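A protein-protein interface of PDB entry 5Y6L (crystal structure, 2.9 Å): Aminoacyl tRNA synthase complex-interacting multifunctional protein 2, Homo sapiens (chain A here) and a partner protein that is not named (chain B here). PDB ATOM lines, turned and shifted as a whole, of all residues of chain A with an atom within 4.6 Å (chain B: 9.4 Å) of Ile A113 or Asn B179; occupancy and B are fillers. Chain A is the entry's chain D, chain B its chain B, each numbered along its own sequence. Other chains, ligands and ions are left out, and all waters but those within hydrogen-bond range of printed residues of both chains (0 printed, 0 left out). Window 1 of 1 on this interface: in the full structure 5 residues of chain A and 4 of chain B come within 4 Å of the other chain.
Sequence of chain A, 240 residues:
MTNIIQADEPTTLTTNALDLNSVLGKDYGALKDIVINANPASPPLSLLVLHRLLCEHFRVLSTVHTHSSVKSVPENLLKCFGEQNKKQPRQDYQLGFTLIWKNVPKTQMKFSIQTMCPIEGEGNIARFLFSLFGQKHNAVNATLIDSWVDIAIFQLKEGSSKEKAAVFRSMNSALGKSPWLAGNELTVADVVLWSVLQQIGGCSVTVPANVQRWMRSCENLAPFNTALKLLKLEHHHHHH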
ATOM      1  N   PHE A 111      29.175  33.114   5.592  1.00  0.00           N
ATOM      2  CA  PHE A 111      29.873  33.017   6.843  1.00  0.00           C
ATOM      3  C   PHE A 111      30.379  31.614   7.127  1.00  0.00           C
ATOM      4  O   PHE A 111      31.523  31.318   6.915  1.00  0.00           O
ATOM      5  CB  PHE A 111      28.953  33.496   7.929  1.00  0.00           C
ATOM      6  CG  PHE A 111      29.513  33.385   9.282  1.00  0.00           C
ATOM      7  CD1 PHE A 111      30.794  33.740   9.529  1.00  0.00           C
ATOM      8  CD2 PHE A 111      28.739  32.935  10.307  1.00  0.00           C
ATOM      9  CE1 PHE A 111      31.308  33.635  10.787  1.00  0.00           C
ATOM     10  CE2 PHE A 111      29.235  32.829  11.569  1.00  0.00           C
ATOM     11  CZ  PHE A 111      30.528  33.178  11.811  1.00  0.00           C
ATOM     12  N   SER A 112      29.511  30.739   7.582  1.00  0.00           N
ATOM     13  CA  SER A 112      29.896  29.379   7.938  1.00  0.00           C
ATOM     14  C   SER A 112      29.570  28.468   6.757  1.00  0.00           C
ATOM     15  O   SER A 112      28.466  27.942   6.646  1.00  0.00           O
ATOM     16  CB  SER A 112      29.201  28.933   9.220  1.00  0.00           C
ATOM     17  OG  SER A 112      29.652  27.651   9.617  1.00  0.00           O
ATOM     18  N   ILE A 113      30.557  28.274   5.885  1.00  0.00           N
ATOM     19  CA  ILE A 113      30.412  27.453   4.688  1.00  0.00           C
ATOM     20  C   ILE A 113      29.911  26.040   4.996  1.00  0.00           C
ATOM     21  O   ILE A 113      29.289  25.399   4.134  1.00  0.00           O
ATOM     22  CB  ILE A 113      31.769  27.457   3.940  1.00  0.00           C
ATOM     23  CG1 ILE A 113      31.952  28.783   3.194  1.00  0.00           C
ATOM     24  CG2 ILE A 113      31.956  26.240   3.027  1.00  0.00           C
ATOM     25  CD1 ILE A 113      30.758  29.167   2.340  1.00  0.00           C
ATOM     26  N   GLN A 114      30.170  25.517   6.203  1.00  0.00           N
ATOM     27  CA  GLN A 114      29.837  24.113   6.429  1.00  0.00           C
ATOM     28  C   GLN A 114      28.384  23.923   6.849  1.00  0.00           C
ATOM     29  O   GLN A 114      27.746  22.941   6.429  1.00  0.00           O
ATOM     30  CB  GLN A 114      30.750  23.486   7.483  1.00  0.00           C
ATOM     31  CG  GLN A 114      30.344  22.038   7.838  1.00  0.00           C
ATOM     32  CD  GLN A 114      30.155  21.691   9.343  1.00  0.00           C
ATOM     33  OE1 GLN A 114      29.385  20.795   9.706  1.00  0.00           O
ATOM     34  NE2 GLN A 114      30.876  22.418  10.212  1.00  0.00           N
ATOM     35  N   THR A 115      27.837  24.859   7.643  1.00  0.00           N
ATOM     36  CA  THR A 115      26.476  24.726   8.134  1.00  0.00           C
ATOM     37  C   THR A 115      25.486  25.714   7.516  1.00  0.00           C
ATOM     38  O   THR A 115      24.361  25.324   7.214  1.00  0.00           O
ATOM     39  CB  THR A 115      26.490  24.846   9.662  1.00  0.00           C
ATOM     40  OG1 THR A 115      26.954  26.135  10.066  1.00  0.00           O
ATOM     41  CG2 THR A 115      27.436  23.825  10.268  1.00  0.00           C
ATOM     42  N   MET A 116      25.882  26.958   7.258  1.00  0.00           N
ATOM     43  CA  MET A 116      24.944  27.990   6.827  1.00  0.00           C
ATOM     44  C   MET A 116      24.801  28.032   5.315  1.00  0.00           C
ATOM     45  O   MET A 116      25.796  28.021   4.587  1.00  0.00           O
ATOM     46  CB  MET A 116      25.389  29.373   7.285  1.00  0.00           C
ATOM     47  CG  MET A 116      25.705  29.497   8.746  1.00  0.00           C
ATOM     48  SD  MET A 116      25.658  31.244   9.157  1.00  0.00           S
ATOM     49  CE  MET A 116      24.008  31.657   8.646  1.00  0.00           C
ATOM     50  N   CYS A 117      23.574  28.126   4.841  1.00  0.00           N
ATOM     51  CA  CYS A 117      23.400  28.600   3.492  1.00  0.00           C
ATOM     52  C   CYS A 117      23.782  30.081   3.445  1.00  0.00           C
ATOM     53  O   CYS A 117      23.811  30.760   4.480  1.00  0.00           O
ATOM     54  CB  CYS A 117      21.955  28.383   3.036  1.00  0.00           C
ATOM     55  SG  CYS A 117      20.700  29.362   3.914  1.00  0.00           S
ATOM     56  N   PRO A 118      24.107  30.607   2.266  1.00  0.00           N
ATOM     57  CA  PRO A 118      24.375  32.041   2.180  1.00  0.00           C
ATOM     58  C   PRO A 118      23.095  32.803   2.455  1.00  0.00           C
ATOM     59  O   PRO A 118      21.999  32.358   2.112  1.00  0.00           O
ATOM     60  CB  PRO A 118      24.881  32.234   0.744  1.00  0.00           C
ATOM     61  CG  PRO A 118      24.313  31.120   0.008  1.00  0.00           C
ATOM     62  CD  PRO A 118      24.250  29.956   0.956  1.00  0.00           C
ATOM     63  N   VAL B 145      35.438  14.508   1.072  1.00  0.00           N
ATOM     64  CA  VAL B 145      34.396  15.500   0.841  1.00  0.00           C
ATOM     65  C   VAL B 145      33.837  15.340  -0.568  1.00  0.00           C
ATOM     66  O   VAL B 145      32.611  15.324  -0.766  1.00  0.00           O
ATOM     67  CB  VAL B 145      34.919  16.929   1.110  1.00  0.00           C
ATOM     68  CG1 VAL B 145      33.915  17.979   0.628  1.00  0.00           C
ATOM     69  CG2 VAL B 145      35.187  17.117   2.586  1.00  0.00           C
ATOM     70  N   LYS B 148      31.496  12.293  -0.694  1.00  0.00           N
ATOM     71  CA  LYS B 148      30.223  12.515  -0.021  1.00  0.00           C
ATOM     72  C   LYS B 148      29.298  13.357  -0.880  1.00  0.00           C
ATOM     73  O   LYS B 148      28.071  13.255  -0.766  1.00  0.00           O
ATOM     74  CB  LYS B 148      30.434  13.178   1.336  1.00  0.00           C
ATOM     75  CG  LYS B 148      30.891  12.261   2.438  1.00  0.00           C
ATOM     76  CD  LYS B 148      31.501  13.135   3.496  1.00  0.00           C
ATOM     77  CE  LYS B 148      32.169  12.356   4.601  1.00  0.00           C
ATOM     78  NZ  LYS B 148      32.846  13.342   5.488  1.00  0.00           N
ATOM     79  N   GLU B 149      29.859  14.187  -1.746  1.00  0.00           N
ATOM     80  CA  GLU B 149      29.033  14.932  -2.675  1.00  0.00           C
ATOM     81  C   GLU B 149      28.718  14.133  -3.933  1.00  0.00           C
ATOM     82  O   GLU B 149      27.664  14.342  -4.535  1.00  0.00           O
ATOM     83  CB  GLU B 149      29.721  16.240  -3.037  1.00  0.00           C
ATOM     84  CG  GLU B 149      28.815  17.206  -3.739  1.00  0.00           C
ATOM     85  CD  GLU B 149      29.389  18.618  -3.813  1.00  0.00           C
ATOM     86  OE1 GLU B 149      29.239  19.247  -4.901  1.00  0.00           O
ATOM     87  OE2 GLU B 149      29.970  19.093  -2.793  1.00  0.00           O
ATOM     88  N   LEU B 152      25.648  12.198  -2.958  1.00  0.00           N
ATOM     89  CA  LEU B 152      25.081  13.269  -2.132  1.00  0.00           C
ATOM     90  C   LEU B 152      23.782  12.856  -1.456  1.00  0.00           C
ATOM     91  O   LEU B 152      23.510  13.302  -0.331  1.00  0.00           O
ATOM     92  CB  LEU B 152      24.846  14.547  -2.950  1.00  0.00           C
ATOM     93  CG  LEU B 152      23.564  14.709  -3.760  1.00  0.00           C
ATOM     94  CD1 LEU B 152      23.479  16.070  -4.365  1.00  0.00           C
ATOM     95  CD2 LEU B 152      23.497  13.640  -4.831  1.00  0.00           C
ATOM     96  N   VAL B 175      31.168  14.343   9.730  1.00  0.00           N
ATOM     97  CA  VAL B 175      30.993  15.730   9.304  1.00  0.00           C
ATOM     98  C   VAL B 175      30.497  15.762   7.869  1.00  0.00           C
ATOM     99  O   VAL B 175      31.096  15.132   6.987  1.00  0.00           O
ATOM    100  CB  VAL B 175      32.321  16.485   9.413  1.00  0.00           C
ATOM    101  CG1 VAL B 175      32.167  17.855   8.838  1.00  0.00           C
ATOM    102  CG2 VAL B 175      32.807  16.512  10.850  1.00  0.00           C
ATOM    103  N   PHE B 176      29.411  16.507   7.623  1.00  0.00           N
ATOM    104  CA  PHE B 176      28.871  16.714   6.279  1.00  0.00           C
ATOM    105  C   PHE B 176      28.775  18.199   6.011  1.00  0.00           C
ATOM    106  O   PHE B 176      28.107  18.917   6.757  1.00  0.00           O
ATOM    107  CB  PHE B 176      27.487  16.085   6.111  1.00  0.00           C
ATOM    108  CG  PHE B 176      27.506  14.596   6.088  1.00  0.00           C
ATOM    109  CD1 PHE B 176      27.766  13.919   4.898  1.00  0.00           C
ATOM    110  CD2 PHE B 176      27.281  13.873   7.263  1.00  0.00           C
ATOM    111  CE1 PHE B 176      27.802  12.550   4.869  1.00  0.00           C
ATOM    112  CE2 PHE B 176      27.314  12.496   7.255  1.00  0.00           C
ATOM    113  CZ  PHE B 176      27.579  11.828   6.054  1.00  0.00           C
ATOM    114  N   ILE B 177      29.446  18.656   4.954  1.00  0.00           N
ATOM    115  CA  ILE B 177      29.261  20.018   4.459  1.00  0.00           C
ATOM    116  C   ILE B 177      27.862  20.135   3.882  1.00  0.00           C
ATOM    117  O   ILE B 177      27.421  19.258   3.125  1.00  0.00           O
ATOM    118  CB  ILE B 177      30.302  20.354   3.383  1.00  0.00           C
ATOM    119  CG1 ILE B 177      31.678  20.571   3.990  1.00  0.00           C
ATOM    120  CG2 ILE B 177      29.924  21.620   2.653  1.00  0.00           C
ATOM    121  CD1 ILE B 177      32.732  20.887   2.928  1.00  0.00           C
ATOM    122  N   LYS B 178      27.158  21.217   4.227  1.00  0.00           N
ATOM    123  CA  LYS B 178      25.786  21.402   3.758  1.00  0.00           C
ATOM    124  C   LYS B 178      25.679  22.266   2.499  1.00  0.00           C
ATOM    125  O   LYS B 178      24.593  22.356   1.919  1.00  0.00           O
ATOM    126  CB  LYS B 178      24.900  21.992   4.878  1.00  0.00           C
ATOM    127  CG  LYS B 178      24.665  21.074   6.091  1.00  0.00           C
ATOM    128  CD  LYS B 178      24.275  19.678   5.629  1.00  0.00           C
ATOM    129  CE  LYS B 178      23.922  18.771   6.800  1.00  0.00           C
ATOM    130  NZ  LYS B 178      23.281  17.509   6.326  1.00  0.00           N
ATOM    131  N   ASN B 179      26.756  22.893   2.058  1.00  0.00           N
ATOM    132  CA  ASN B 179      26.781  23.596   0.786  1.00  0.00           C
ATOM    133  C   ASN B 179      27.486  22.732  -0.249  1.00  0.00           C
ATOM    134  O   ASN B 179      28.311  21.878   0.078  1.00  0.00           O
ATOM    135  CB  ASN B 179      27.490  24.945   0.919  1.00  0.00           C
ATOM    136  CG  ASN B 179      26.618  26.000   1.565  1.00  0.00           C
ATOM    137  OD1 ASN B 179      25.466  26.213   1.166  1.00  0.00           O
ATOM    138  ND2 ASN B 179      27.159  26.676   2.564  1.00  0.00           N
ATOM    139  N   ARG B 180      27.165  22.946  -1.509  1.00  0.00           N
ATOM    140  CA  ARG B 180      27.814  22.166  -2.552  1.00  0.00           C
ATOM    141  C   ARG B 180      29.132  22.814  -2.985  1.00  0.00           C
ATOM    142  O   ARG B 180      29.202  24.029  -3.233  1.00  0.00           O
ATOM    143  CB  ARG B 180      26.857  21.978  -3.725  1.00  0.00           C
ATOM    144  CG  ARG B 180      25.722  21.070  -3.354  1.00  0.00           C
ATOM    145  CD  ARG B 180      25.836  19.738  -4.055  1.00  0.00           C
ATOM    146  NE  ARG B 180      25.178  19.796  -5.350  1.00  0.00           N
ATOM    147  CZ  ARG B 180      25.540  19.053  -6.385  1.00  0.00           C
ATOM    148  NH1 ARG B 180      26.567  18.210  -6.259  1.00  0.00           N
ATOM    149  NH2 ARG B 180      24.893  19.161  -7.543  1.00  0.00           N
ATOM    150  N   LEU B 181      30.178  21.988  -3.077  1.00  0.00           N
ATOM    151  CA  LEU B 181      31.496  22.450  -3.488  1.00  0.00           C
ATOM    152  C   LEU B 181      31.916  22.010  -4.880  1.00  0.00           C
ATOM    153  O   LEU B 181      32.957  22.474  -5.345  1.00  0.00           O
ATOM    154  CB  LEU B 181      32.577  21.969  -2.506  1.00  0.00           C
ATOM    155  CG  LEU B 181      32.456  22.432  -1.060  1.00  0.00           C
ATOM    156  CD1 LEU B 181      33.708  22.113  -0.320  1.00  0.00           C
ATOM    157  CD2 LEU B 181      32.168  23.924  -0.994  1.00  0.00           C
ATOM    158  N   TYR B 182      31.169  21.138  -5.563  1.00  0.00           N
ATOM    159  CA  TYR B 182      31.716  20.529  -6.771  1.00  0.00           C
ATOM    160  C   TYR B 182      30.837  20.546  -8.019  1.00  0.00           C
ATOM    161  O   TYR B 182      31.340  20.179  -9.085  1.00  0.00           O
ATOM    162  CB  TYR B 182      32.119  19.071  -6.500  1.00  0.00           C
ATOM    163  CG  TYR B 182      33.295  18.897  -5.545  1.00  0.00           C
ATOM    164  CD1 TYR B 182      34.623  18.857  -6.015  1.00  0.00           C
ATOM    165  CD2 TYR B 182      33.077  18.748  -4.166  1.00  0.00           C
ATOM    166  CE1 TYR B 182      35.697  18.688  -5.129  1.00  0.00           C
ATOM    167  CE2 TYR B 182      34.134  18.575  -3.273  1.00  0.00           C
ATOM    168  CZ  TYR B 182      35.440  18.544  -3.754  1.00  0.00           C
ATOM    169  OH  TYR B 182      36.470  18.365  -2.840  1.00  0.00           O
ATOM    170  N   THR B 183      29.567  20.930  -7.951  1.00  0.00           N
ATOM    171  CA  THR B 183      28.728  20.761  -9.134  1.00  0.00           C
ATOM    172  C   THR B 183      27.533  21.713  -9.053  1.00  0.00           C
ATOM    173  O   THR B 183      27.217  22.271  -7.991  1.00  0.00           O
ATOM    174  CB  THR B 183      28.231  19.303  -9.292  1.00  0.00           C
ATOM    175  OG1 THR B 183      29.214  18.366  -8.852  1.00  0.00           O
ATOM    176  CG2 THR B 183      27.869  18.990 -10.766  1.00  0.00           C
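The backbone carbonyl oxygen of Met A116 is in hydrogen-bond range of the side-chain amide nitrogen of Asn B179 (2.8 Å). The backbone carbonyl oxygen (O) of Ile A113 lies within hydrogen-bond range of the side-chain amide nitrogen (ND2) of Asn B179, 2.9 Å away. O of Gln A114 sits at hydrogen-bond distance from N of Lys B178 (2.9 Å).
Phe B176 touches Gln A114 (O to OE1, 3.7 Å). Gln A114 touches Ile B177 (O to C, 3.8 Å). Asn B179 touches Cys A117. Pro A118 touches Asn B179.
No residue of chain B comes within 4 Å of Ser A112. Of chain B, only Asn B179 comes within 4 Å of Ile A113. Of the printed residues of chain B, Met A116 touches Asn B179. Of the printed residues of chain B, Pro A118 touches Asn B179 (3.9 Å). Printed residues of chain A within 4 Å of Phe B176: Gln A114. Of chain A, only Ile A113, Met A116, Cys A117 and Pro A118 come within 4 Å of Asn B179. The nearest printed residue of chain A that does not touch Asn B179 is Ser A112 (4.5 Å). The nearest printed residue of chain A that does not touch Lys B178 is Thr A115 (4.1 Å).
Hydrophobic or aromatic side chains of chain A that line the printed part of chain B: Pro A118. Along chain A the printed residues that touch a printed residue of chain B span positions 113 to 118. Among the printed residues, 7 pairs touch across the chains. Among the printed residues, no Asp or Glu carboxylate lies within 4 Å of a Lys or Arg side-chain nitrogen of the other chain.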
